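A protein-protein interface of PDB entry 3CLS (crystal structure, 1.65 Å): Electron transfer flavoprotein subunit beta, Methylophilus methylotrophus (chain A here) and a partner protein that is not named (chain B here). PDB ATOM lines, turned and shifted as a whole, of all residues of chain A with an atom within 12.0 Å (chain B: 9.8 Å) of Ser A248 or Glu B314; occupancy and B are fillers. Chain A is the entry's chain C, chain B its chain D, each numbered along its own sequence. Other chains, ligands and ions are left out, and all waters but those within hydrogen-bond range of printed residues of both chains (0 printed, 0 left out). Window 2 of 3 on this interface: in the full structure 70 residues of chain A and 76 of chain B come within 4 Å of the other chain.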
ATOM      1  N   ILE A 243       4.989  14.417  -0.066  1.00  0.00           N
ATOM      2  CA  ILE A 243       6.422  14.280  -0.211  1.00  0.00           C
ATOM      3  C   ILE A 243       6.693  14.366  -1.699  1.00  0.00           C
ATOM      4  O   ILE A 243       6.290  13.499  -2.476  1.00  0.00           O
ATOM      5  CB  ILE A 243       6.945  12.974   0.427  1.00  0.00           C
ATOM      6  CG1 ILE A 243       6.469  12.842   1.872  1.00  0.00           C
ATOM      7  CG2 ILE A 243       8.476  12.881   0.394  1.00  0.00           C
ATOM      8  CD1 ILE A 243       6.230  11.437   2.262  1.00  0.00           C
ATOM      9  N   GLU A 244       7.344  15.461  -2.077  1.00  0.00           N
ATOM     10  CA  GLU A 244       7.639  15.769  -3.482  1.00  0.00           C
ATOM     11  C   GLU A 244       8.987  15.156  -3.830  1.00  0.00           C
ATOM     12  O   GLU A 244       9.591  14.475  -3.008  1.00  0.00           O
ATOM     13  CB  GLU A 244       7.636  17.297  -3.698  1.00  0.00           C
ATOM     14  CG  GLU A 244       6.262  17.911  -3.430  1.00  0.00           C
ATOM     15  CD  GLU A 244       6.093  19.344  -3.953  1.00  0.00           C
ATOM     16  OE1 GLU A 244       7.025  20.165  -3.881  1.00  0.00           O
ATOM     17  OE2 GLU A 244       4.956  19.641  -4.415  1.00  0.00           O
ATOM     18  N   GLY A 245       9.490  15.438  -5.020  1.00  0.00           N
ATOM     19  CA  GLY A 245      10.855  15.036  -5.376  1.00  0.00           C
ATOM     20  C   GLY A 245      10.959  13.650  -5.979  1.00  0.00           C
ATOM     21  O   GLY A 245       9.969  13.068  -6.413  1.00  0.00           O
ATOM     22  N   THR A 246      12.177  13.128  -5.997  1.00  0.00           N
ATOM     23  CA  THR A 246      12.438  11.846  -6.685  1.00  0.00           C
ATOM     24  C   THR A 246      11.877  10.623  -5.975  1.00  0.00           C
ATOM     25  O   THR A 246      11.564  10.634  -4.792  1.00  0.00           O
ATOM     26  CB  THR A 246      13.925  11.633  -6.908  1.00  0.00           C
ATOM     27  OG1 THR A 246      14.575  11.345  -5.667  1.00  0.00           O
ATOM     28  CG2 THR A 246      14.567  12.825  -7.549  1.00  0.00           C
ATOM     29  N   ILE A 247      11.747   9.524  -6.721  1.00  0.00           N
ATOM     30  CA  ILE A 247      11.379   8.301  -6.121  1.00  0.00           C
ATOM     31  C   ILE A 247      12.327   7.904  -5.000  1.00  0.00           C
ATOM     32  O   ILE A 247      11.851   7.345  -4.002  1.00  0.00           O
ATOM     33  CB  ILE A 247      11.403   7.147  -7.206  1.00  0.00           C
ATOM     34  CG1 ILE A 247      10.218   7.293  -8.156  1.00  0.00           C
ATOM     35  CG2 ILE A 247      11.378   5.761  -6.532  1.00  0.00           C
ATOM     36  CD1 ILE A 247       8.846   6.945  -7.540  1.00  0.00           C
ATOM     37  N   SER A 248      13.628   8.166  -5.167  1.00  0.00           N
ATOM     38  CA  SER A 248      14.658   7.765  -4.181  1.00  0.00           C
ATOM     39  C   SER A 248      14.351   8.492  -2.864  1.00  0.00           C
ATOM     40  O   SER A 248      14.332   7.885  -1.797  1.00  0.00           O
ATOM     41  CB  SER A 248      16.114   8.032  -4.661  1.00  0.00           C
ATOM     42  N   GLU A 249      14.020   9.767  -2.967  1.00  0.00           N
ATOM     43  CA  GLU A 249      13.760  10.548  -1.740  1.00  0.00           C
ATOM     44  C   GLU A 249      12.428  10.359  -1.136  1.00  0.00           C
ATOM     45  O   GLU A 249      12.325  10.412   0.084  1.00  0.00           O
ATOM     46  CB  GLU A 249      14.062  12.012  -1.908  1.00  0.00           C
ATOM     47  CG  GLU A 249      13.290  12.789  -2.963  1.00  0.00           C
ATOM     48  CD  GLU A 249      14.302  13.751  -3.564  1.00  0.00           C
ATOM     49  OE1 GLU A 249      15.444  13.483  -3.265  1.00  0.00           O
ATOM     50  OE2 GLU A 249      13.969  14.701  -4.306  1.00  0.00           O
ATOM     51  N   GLN A 250      11.408  10.092  -1.969  1.00  0.00           N
ATOM     52  CA  GLN A 250      10.119   9.664  -1.461  1.00  0.00           C
ATOM     53  C   GLN A 250      10.280   8.362  -0.684  1.00  0.00           C
ATOM     54  O   GLN A 250       9.745   8.213   0.414  1.00  0.00           O
ATOM     55  CB  GLN A 250       9.126   9.519  -2.595  1.00  0.00           C
ATOM     56  CG  GLN A 250       8.695  10.849  -3.162  1.00  0.00           C
ATOM     57  CD  GLN A 250       7.962  10.766  -4.458  1.00  0.00           C
ATOM     58  OE1 GLN A 250       8.215   9.872  -5.282  1.00  0.00           O
ATOM     59  NE2 GLN A 250       7.038  11.708  -4.668  1.00  0.00           N
ATOM     60  N   ALA A 251      11.046   7.408  -1.229  1.00  0.00           N
ATOM     61  CA  ALA A 251      11.272   6.165  -0.506  1.00  0.00           C
ATOM     62  C   ALA A 251      12.092   6.403   0.758  1.00  0.00           C
ATOM     63  O   ALA A 251      11.874   5.714   1.747  1.00  0.00           O
ATOM     64  CB  ALA A 251      11.970   5.122  -1.396  1.00  0.00           C
ATOM     65  N   ALA A 252      13.044   7.336   0.692  1.00  0.00           N
ATOM     66  CA  ALA A 252      13.917   7.698   1.813  1.00  0.00           C
ATOM     67  C   ALA A 252      13.064   8.245   2.988  1.00  0.00           C
ATOM     68  O   ALA A 252      13.314   7.927   4.158  1.00  0.00           O
ATOM     69  CB  ALA A 252      14.954   8.744   1.366  1.00  0.00           C
ATOM     70  N   LYS A 253      12.112   9.091   2.668  1.00  0.00           N
ATOM     71  CA  LYS A 253      11.159   9.605   3.681  1.00  0.00           C
ATOM     72  C   LYS A 253      10.279   8.502   4.306  1.00  0.00           C
ATOM     73  O   LYS A 253      10.120   8.460   5.503  1.00  0.00           O
ATOM     74  CB  LYS A 253      10.323  10.739   3.092  1.00  0.00           C
ATOM     75  CG  LYS A 253       9.372  11.442   4.096  1.00  0.00           C
ATOM     76  CD  LYS A 253      10.075  11.975   5.308  1.00  0.00           C
ATOM     77  CE  LYS A 253       9.082  12.783   6.170  1.00  0.00           C
ATOM     78  NZ  LYS A 253       9.703  13.285   7.384  1.00  0.00           N
ATOM     79  N   ILE A 254       9.778   7.572   3.505  1.00  0.00           N
ATOM     80  CA  ILE A 254       9.001   6.434   3.997  1.00  0.00           C
ATOM     81  C   ILE A 254       9.837   5.673   4.993  1.00  0.00           C
ATOM     82  O   ILE A 254       9.391   5.383   6.102  1.00  0.00           O
ATOM     83  CB  ILE A 254       8.495   5.491   2.841  1.00  0.00           C
ATOM     84  CG1 ILE A 254       7.435   6.188   1.992  1.00  0.00           C
ATOM     85  CG2 ILE A 254       7.853   4.232   3.386  1.00  0.00           C
ATOM     86  CD1 ILE A 254       7.128   5.531   0.727  1.00  0.00           C
ATOM     87  N   ILE A 255      11.090   5.382   4.643  1.00  0.00           N
ATOM     88  CA  ILE A 255      11.908   4.596   5.549  1.00  0.00           C
ATOM     89  C   ILE A 255      12.150   5.327   6.871  1.00  0.00           C
ATOM     90  O   ILE A 255      12.176   4.706   7.929  1.00  0.00           O
ATOM     91  CB  ILE A 255      13.211   4.164   4.881  1.00  0.00           C
ATOM     92  CG1 ILE A 255      12.874   3.137   3.784  1.00  0.00           C
ATOM     93  CG2 ILE A 255      14.210   3.622   5.922  1.00  0.00           C
ATOM     94  CD1 ILE A 255      14.110   2.492   3.117  1.00  0.00           C
ATOM     95  N   GLN A 256      12.342   6.637   6.807  1.00  0.00           N
ATOM     96  CA  GLN A 256      12.510   7.438   8.009  1.00  0.00           C
ATOM     97  C   GLN A 256      11.238   7.409   8.862  1.00  0.00           C
ATOM     98  O   GLN A 256      11.323   7.296  10.083  1.00  0.00           O
ATOM     99  CB  GLN A 256      12.832   8.870   7.646  1.00  0.00           C
ATOM    100  CG  GLN A 256      14.143   9.039   6.939  1.00  0.00           C
ATOM    101  CD  GLN A 256      14.668  10.427   7.110  1.00  0.00           C
ATOM    102  OE1 GLN A 256      15.899  10.679   7.094  1.00  0.00           O
ATOM    103  NE2 GLN A 256      13.728  11.364   7.313  1.00  0.00           N
ATOM    104  N   ILE A 257      10.081   7.505   8.210  1.00  0.00           N
ATOM    105  CA  ILE A 257       8.777   7.317   8.886  1.00  0.00           C
ATOM    106  C   ILE A 257       8.694   5.917   9.527  1.00  0.00           C
ATOM    107  O   ILE A 257       8.388   5.797  10.725  1.00  0.00           O
ATOM    108  CB  ILE A 257       7.594   7.620   7.961  1.00  0.00           C
ATOM    109  CG1 ILE A 257       7.715   9.059   7.446  1.00  0.00           C
ATOM    110  CG2 ILE A 257       6.258   7.425   8.698  1.00  0.00           C
ATOM    111  CD1 ILE A 257       6.923   9.400   6.208  1.00  0.00           C
ATOM    112  N   ILE A 258       9.061   4.869   8.781  1.00  0.00           N
ATOM    113  CA  ILE A 258       9.140   3.508   9.363  1.00  0.00           C
ATOM    114  C   ILE A 258      10.084   3.407  10.548  1.00  0.00           C
ATOM    115  O   ILE A 258       9.795   2.712  11.529  1.00  0.00           O
ATOM    116  CB  ILE A 258       9.539   2.428   8.310  1.00  0.00           C
ATOM    117  CG1 ILE A 258       8.429   2.310   7.240  1.00  0.00           C
ATOM    118  CG2 ILE A 258       9.795   1.088   8.989  1.00  0.00           C
ATOM    119  CD1 ILE A 258       8.893   1.751   5.863  1.00  0.00           C
ATOM    120  N   ASN A 259      11.244   4.048  10.434  1.00  0.00           N
ATOM    121  CA  ASN A 259      12.243   4.004  11.477  1.00  0.00           C
ATOM    122  C   ASN A 259      11.794   4.792  12.716  1.00  0.00           C
ATOM    123  O   ASN A 259      11.973   4.333  13.839  1.00  0.00           O
ATOM    124  CB  ASN A 259      13.582   4.535  10.953  1.00  0.00           C
ATOM    125  CG  ASN A 259      14.334   3.515  10.092  1.00  0.00           C
ATOM    126  OD1 ASN A 259      14.058   2.316  10.133  1.00  0.00           O
ATOM    127  ND2 ASN A 259      15.316   4.000   9.336  1.00  0.00           N
ATOM    128  N   GLN B 221       5.751  -9.258  -5.050  1.00  0.00           N
ATOM    129  CA  GLN B 221       6.738  -8.248  -4.761  1.00  0.00           C
ATOM    130  C   GLN B 221       6.360  -7.396  -3.546  1.00  0.00           C
ATOM    131  O   GLN B 221       7.236  -6.928  -2.823  1.00  0.00           O
ATOM    132  CB  GLN B 221       7.001  -7.360  -5.994  1.00  0.00           C
ATOM    133  CG  GLN B 221       5.829  -6.466  -6.469  1.00  0.00           C
ATOM    134  CD  GLN B 221       6.054  -5.989  -7.886  1.00  0.00           C
ATOM    135  OE1 GLN B 221       5.809  -6.729  -8.851  1.00  0.00           O
ATOM    136  NE2 GLN B 221       6.547  -4.780  -8.030  1.00  0.00           N
ATOM    137  N   PHE B 222       5.066  -7.212  -3.337  1.00  0.00           N
ATOM    138  CA  PHE B 222       4.573  -6.523  -2.125  1.00  0.00           C
ATOM    139  C   PHE B 222       4.634  -7.403  -0.889  1.00  0.00           C
ATOM    140  O   PHE B 222       4.912  -6.911   0.191  1.00  0.00           O
ATOM    141  CB  PHE B 222       3.200  -5.925  -2.328  1.00  0.00           C
ATOM    142  CG  PHE B 222       3.210  -4.830  -3.321  1.00  0.00           C
ATOM    143  CD1 PHE B 222       3.008  -5.111  -4.678  1.00  0.00           C
ATOM    144  CD2 PHE B 222       3.468  -3.514  -2.943  1.00  0.00           C
ATOM    145  CE1 PHE B 222       3.085  -4.095  -5.633  1.00  0.00           C
ATOM    146  CE2 PHE B 222       3.547  -2.490  -3.926  1.00  0.00           C
ATOM    147  CZ  PHE B 222       3.342  -2.801  -5.252  1.00  0.00           C
ATOM    148  N   LEU B 225       8.194  -7.130   0.041  1.00  0.00           N
ATOM    149  CA  LEU B 225       8.417  -5.814   0.656  1.00  0.00           C
ATOM    150  C   LEU B 225       7.975  -5.823   2.118  1.00  0.00           C
ATOM    151  O   LEU B 225       8.739  -5.408   2.988  1.00  0.00           O
ATOM    152  CB  LEU B 225       7.707  -4.707  -0.142  1.00  0.00           C
ATOM    153  CG  LEU B 225       7.722  -3.289   0.444  1.00  0.00           C
ATOM    154  CD1 LEU B 225       9.121  -2.776   0.672  1.00  0.00           C
ATOM    155  CD2 LEU B 225       6.896  -2.343  -0.459  1.00  0.00           C
ATOM    156  N   GLU B 228      10.340  -7.762   4.064  1.00  0.00           N
ATOM    157  CA  GLU B 228      11.624  -7.063   4.263  1.00  0.00           C
ATOM    158  C   GLU B 228      11.470  -5.935   5.294  1.00  0.00           C
ATOM    159  O   GLU B 228      12.394  -5.635   6.057  1.00  0.00           O
ATOM    160  CB  GLU B 228      12.164  -6.504   2.941  1.00  0.00           C
ATOM    161  N   ILE B 304       2.267  10.295  -1.028  1.00  0.00           N
ATOM    162  CA  ILE B 304       3.235  10.252  -2.084  1.00  0.00           C
ATOM    163  C   ILE B 304       2.474   9.982  -3.381  1.00  0.00           C
ATOM    164  O   ILE B 304       1.870   8.906  -3.526  1.00  0.00           O
ATOM    165  CB  ILE B 304       4.243   9.124  -1.865  1.00  0.00           C
ATOM    166  CG1 ILE B 304       5.135   9.399  -0.650  1.00  0.00           C
ATOM    167  CG2 ILE B 304       5.159   8.968  -3.080  1.00  0.00           C
ATOM    168  CD1 ILE B 304       4.548   8.784   0.628  1.00  0.00           C
ATOM    169  N   ALA B 306       2.934   8.884  -6.510  1.00  0.00           N
ATOM    170  CA  ALA B 306       3.910   8.175  -7.317  1.00  0.00           C
ATOM    171  C   ALA B 306       3.443   6.758  -7.592  1.00  0.00           C
ATOM    172  O   ALA B 306       2.614   6.220  -6.868  1.00  0.00           O
ATOM    173  CB  ALA B 306       5.258   8.106  -6.641  1.00  0.00           C
ATOM    174  N   ASP B 307       4.057   6.183  -8.625  1.00  0.00           N
ATOM    175  CA  ASP B 307       3.831   4.833  -9.011  1.00  0.00           C
ATOM    176  C   ASP B 307       4.242   3.843  -7.908  1.00  0.00           C
ATOM    177  O   ASP B 307       5.357   3.883  -7.378  1.00  0.00           O
ATOM    178  CB  ASP B 307       4.532   4.522 -10.333  1.00  0.00           C
ATOM    179  CG  ASP B 307       4.280   3.095 -10.804  1.00  0.00           C
ATOM    180  OD1 ASP B 307       5.137   2.232 -10.495  1.00  0.00           O
ATOM    181  OD2 ASP B 307       3.257   2.847 -11.466  1.00  0.00           O
ATOM    182  N   ILE B 308       3.324   2.942  -7.560  1.00  0.00           N
ATOM    183  CA  ILE B 308       3.577   2.027  -6.430  1.00  0.00           C
ATOM    184  C   ILE B 308       4.691   1.046  -6.721  1.00  0.00           C
ATOM    185  O   ILE B 308       5.381   0.649  -5.818  1.00  0.00           O
ATOM    186  CB  ILE B 308       2.281   1.261  -5.905  1.00  0.00           C
ATOM    187  CG1 ILE B 308       1.541   0.553  -7.034  1.00  0.00           C
ATOM    188  CG2 ILE B 308       1.395   2.255  -5.166  1.00  0.00           C
ATOM    189  CD1 ILE B 308       0.509  -0.425  -6.508  1.00  0.00           C
ATOM    190  N   PHE B 309       4.824   0.600  -7.977  1.00  0.00           N
ATOM    191  CA  PHE B 309       5.897  -0.342  -8.341  1.00  0.00           C
ATOM    192  C   PHE B 309       7.234   0.375  -8.250  1.00  0.00           C
ATOM    193  O   PHE B 309       8.172  -0.157  -7.677  1.00  0.00           O
ATOM    194  CB  PHE B 309       5.652  -0.973  -9.731  1.00  0.00           C
ATOM    195  CG  PHE B 309       4.230  -1.435  -9.935  1.00  0.00           C
ATOM    196  CD1 PHE B 309       3.364  -0.695 -10.715  1.00  0.00           C
ATOM    197  CD2 PHE B 309       3.738  -2.564  -9.293  1.00  0.00           C
ATOM    198  CE1 PHE B 309       2.038  -1.075 -10.868  1.00  0.00           C
ATOM    199  CE2 PHE B 309       2.408  -2.931  -9.414  1.00  0.00           C
ATOM    200  CZ  PHE B 309       1.573  -2.195 -10.225  1.00  0.00           C
ATOM    201  N   ASP B 310       7.333   1.585  -8.772  1.00  0.00           N
ATOM    202  CA  ASP B 310       8.606   2.330  -8.647  1.00  0.00           C
ATOM    203  C   ASP B 310       8.973   2.569  -7.168  1.00  0.00           C
ATOM    204  O   ASP B 310      10.130   2.415  -6.779  1.00  0.00           O
ATOM    205  CB  ASP B 310       8.511   3.666  -9.364  1.00  0.00           C
ATOM    206  CG  ASP B 310       8.418   3.528 -10.853  1.00  0.00           C
ATOM    207  OD1 ASP B 310       8.753   2.454 -11.378  1.00  0.00           O
ATOM    208  OD2 ASP B 310       7.994   4.504 -11.495  1.00  0.00           O
ATOM    209  N   ILE B 311       7.993   2.939  -6.347  1.00  0.00           N
ATOM    210  CA  ILE B 311       8.256   3.123  -4.921  1.00  0.00           C
ATOM    211  C   ILE B 311       8.630   1.806  -4.237  1.00  0.00           C
ATOM    212  O   ILE B 311       9.574   1.749  -3.477  1.00  0.00           O
ATOM    213  CB  ILE B 311       7.014   3.755  -4.202  1.00  0.00           C
ATOM    214  CG1 ILE B 311       6.816   5.203  -4.673  1.00  0.00           C
ATOM    215  CG2 ILE B 311       7.135   3.636  -2.679  1.00  0.00           C
ATOM    216  CD1 ILE B 311       7.860   6.237  -4.138  1.00  0.00           C
ATOM    217  N   GLU B 312       7.897   0.737  -4.519  1.00  0.00           N
ATOM    218  CA  GLU B 312       8.181  -0.567  -3.904  1.00  0.00           C
ATOM    219  C   GLU B 312       9.626  -1.025  -4.192  1.00  0.00           C
ATOM    220  O   GLU B 312      10.359  -1.439  -3.276  1.00  0.00           O
ATOM    221  CB  GLU B 312       7.134  -1.608  -4.351  1.00  0.00           C
ATOM    222  CG  GLU B 312       7.514  -3.059  -4.003  1.00  0.00           C
ATOM    223  CD  GLU B 312       8.335  -3.738  -5.085  1.00  0.00           C
ATOM    224  OE1 GLU B 312       8.112  -3.465  -6.285  1.00  0.00           O
ATOM    225  OE2 GLU B 312       9.228  -4.529  -4.733  1.00  0.00           O
ATOM    226  N   GLU B 313      10.038  -0.928  -5.454  1.00  0.00           N
ATOM    227  CA  GLU B 313      11.366  -1.403  -5.829  1.00  0.00           C
ATOM    228  C   GLU B 313      12.448  -0.560  -5.166  1.00  0.00           C
ATOM    229  O   GLU B 313      13.471  -1.098  -4.730  1.00  0.00           O
ATOM    230  CB  GLU B 313      11.537  -1.517  -7.341  1.00  0.00           C
ATOM    231  CG  GLU B 313      11.263  -0.264  -8.170  1.00  0.00           C
ATOM    232  CD  GLU B 313      12.112  -0.192  -9.474  1.00  0.00           C
ATOM    233  OE1 GLU B 313      13.251  -0.703  -9.471  1.00  0.00           O
ATOM    234  OE2 GLU B 313      11.634   0.381 -10.498  1.00  0.00           O
ATOM    235  N   GLU B 314      12.203   0.742  -5.033  1.00  0.00           N
ATOM    236  CA  GLU B 314      13.208   1.626  -4.415  1.00  0.00           C
ATOM    237  C   GLU B 314      13.257   1.389  -2.914  1.00  0.00           C
ATOM    238  O   GLU B 314      14.317   1.370  -2.321  1.00  0.00           O
ATOM    239  CB  GLU B 314      12.926   3.082  -4.739  1.00  0.00           C
ATOM    240  CG  GLU B 314      13.869   4.077  -4.150  1.00  0.00           C
ATOM    241  CD  GLU B 314      15.287   4.008  -4.685  1.00  0.00           C
ATOM    242  OE1 GLU B 314      15.487   3.601  -5.859  1.00  0.00           O
ATOM    243  OE2 GLU B 314      16.215   4.378  -3.928  1.00  0.00           O
ATOM    244  N   LEU B 315      12.091   1.179  -2.319  1.00  0.00           N
ATOM    245  CA  LEU B 315      11.968   0.871  -0.907  1.00  0.00           C
ATOM    246  C   LEU B 315      12.738  -0.422  -0.594  1.00  0.00           C
ATOM    247  O   LEU B 315      13.535  -0.444   0.333  1.00  0.00           O
ATOM    248  CB  LEU B 315      10.476   0.722  -0.586  1.00  0.00           C
ATOM    249  CG  LEU B 315       9.892   1.215   0.705  1.00  0.00           C
ATOM    250  CD1 LEU B 315      10.565   2.483   1.270  1.00  0.00           C
ATOM    251  CD2 LEU B 315       8.410   1.376   0.434  1.00  0.00           C
ATOM    252  N   LYS B 316      12.506  -1.472  -1.400  1.00  0.00           N
ATOM    253  CA  LYS B 316      13.230  -2.751  -1.273  1.00  0.00           C
ATOM    254  C   LYS B 316      14.731  -2.539  -1.346  1.00  0.00           C
ATOM    255  O   LYS B 316      15.469  -3.099  -0.537  1.00  0.00           O
ATOM    256  CB  LYS B 316      12.812  -3.779  -2.355  1.00  0.00           C
ATOM    257  N   ALA B 317      15.178  -1.740  -2.311  1.00  0.00           N
ATOM    258  CA  ALA B 317      16.600  -1.499  -2.499  1.00  0.00           C
ATOM    259  C   ALA B 317      17.179  -0.805  -1.280  1.00  0.00           C
ATOM    260  O   ALA B 317      18.166  -1.270  -0.674  1.00  0.00           O
ATOM    261  CB  ALA B 317      16.831  -0.675  -3.760  1.00  0.00           C
ATOM    262  N   GLN B 318      16.556   0.303  -0.905  1.00  0.00           N
ATOM    263  CA  GLN B 318      16.967   1.050   0.270  1.00  0.00           C
ATOM    264  C   GLN B 318      16.910   0.206   1.544  1.00  0.00           C
ATOM    265  O   GLN B 318      17.822   0.293   2.366  1.00  0.00           O
ATOM    266  CB  GLN B 318      16.147   2.332   0.413  1.00  0.00           C
ATOM    267  CG  GLN B 318      16.486   3.357  -0.649  1.00  0.00           C
ATOM    268  CD  GLN B 318      15.910   4.741  -0.393  1.00  0.00           C
ATOM    269  OE1 GLN B 318      15.657   5.140   0.758  1.00  0.00           O
ATOM    270  NE2 GLN B 318      15.763   5.512  -1.465  1.00  0.00           N
ATOM    271  N   LEU B 319      15.887  -0.621   1.723  1.00  0.00           N
ATOM    272  CA  LEU B 319      15.862  -1.536   2.868  1.00  0.00           C
ATOM    273  C   LEU B 319      16.881  -2.644   2.631  1.00  0.00           C
ATOM    274  O   LEU B 319      17.831  -2.761   3.383  1.00  0.00           O
ATOM    275  CB  LEU B 319      14.483  -2.157   3.114  1.00  0.00           C
ATOM    276  CG  LEU B 319      13.330  -1.344   3.677  1.00  0.00           C
ATOM    277  CD1 LEU B 319      12.025  -2.082   3.391  1.00  0.00           C
ATOM    278  CD2 LEU B 319      13.455  -1.092   5.173  1.00  0.00           C
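The backbone NH (N) of Ala A252 sits close to the side-chain amide oxygen (OE1) of Gln B318, at 3.4 Å. The side-chain amide nitrogen of Gln B318 lies within hydrogen-bond range of the backbone carbonyl oxygen of Ser A248, 2.8 Å away.
OD1 of Asp B307 lies within hydrogen-bond range of N of Asp B310, at 2.9 Å. OE2 of Glu B314 sits at hydrogen-bond distance from NE2 of Gln B318. O of Ile A243 is in hydrogen-bond range of NE2 of Gln A250, at 2.9 Å. The backbone NH (N) of Ser A248 sits close to the side-chain hydroxyl (OG1) of Thr A246. The backbone carbonyl oxygen (O) of Thr A246 lies close to the side-chain amide oxygen (OE1) of Gln A250, at 3.5 Å.
Ile A247 touches Ala B306 (CD1 to CB, 3.9 Å). CG2 of Ile A247 touches CB of Glu B314, 3.6 Å away. OE2 of Glu B314 touches CB of Ser A248, at 3.7 Å. Ile B304 touches Gln A250 (CG2 to CD, 3.6 Å). Ala A251 touches Glu B314. Leu B315 touches Ala A251. CG2 of Ile B311 touches CD1 of Ile A254, at 3.9 Å. CD1 of Leu B315 touches CG2 of Ile A254, 3.9 Å away. Ile A255 touches Gln B318 (CD1 to CB, 3.4 Å). CD1 of Ile A255 touches N of Leu B319 (3.8 Å).
Printed residues of chain B within 4 Å of Ile A243: Ile B304. Glu A244 touches none of the printed residues of chain B. No residue of chain B comes within 4 Å of Thr A246. Ile A247 touches just these residues of chain B: Ala B306 (3.9 Å), Asp B310 (3.6 Å), Ile B311 (3.6 Å) and Glu B314 (3.6 Å). Of chain B, only Glu B314 and Gln B318 come within 4 Å of Ser A248. Printed residues of chain B within 4 Å of Gln A250: Ile B304, Ala B306 and Ile B311. Ala A251 touches just these residues of chain B: Glu B314, Leu B315 and Gln B318. Of the printed residues of chain B, Ala A252 touches Gln B318. Printed residues of chain B within 4 Å of Ile A255: Leu B315, Gln B318 and Leu B319. Of the printed residues of chain A, Ile B304 touches Ile A243 (3.5 Å) and Gln A250 (3.6 Å). Of chain A, only Ile A247 (3.6 Å), Gln A250 (3.8 Å) and Ile A254 (3.9 Å) come within 4 Å of Ile B311. No residue of chain A comes within 4 Å of Glu B312. No residue of chain A comes within 4 Å of Glu B313. Printed residues of chain A within 4 Å of Glu B314: Ile A247 (3.6 Å), Ser A248 (3.7 Å) and Ala A251 (3.5 Å). Of chain A, only Ala A251 (3.5 Å), Ile A254 (3.9 Å) and Ile A255 (3.5 Å) come within 4 Å of Leu B315. No residue of chain A comes within 4 Å of Lys B316. Of chain A, only Ser A248 (2.8 Å), Ala A251 (3.8 Å), Ala A252 (3.3 Å) and Ile A255 (3.4 Å) come within 4 Å of Gln B318. The nearest residue of chain A that does not touch Glu B314 is Ile A255 (5.6 Å).
Of the 17 printed residues of chain A, 8 touch a printed residue of chain B. Printed residues of chain A that touch a printed residue of chain B: Ile A243, Ile A247, Ser A248, Gln A250, Ala A251, Ala A252, Ile A254 and Ile A255. Of the 19 printed residues of chain B, 8 touch a printed residue of chain A. Printed residues of chain B that touch a printed residue of chain A: Ile B304, Ala B306, Asp B310, Ile B311, Glu B314, Leu B315, Gln B318 and Leu B319. Hydrophobic or aromatic side chains of chain B within 4 Å of the printed part of chain A: Ile B304, Ala B306, Ile B311, Leu B315 and Leu B319.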
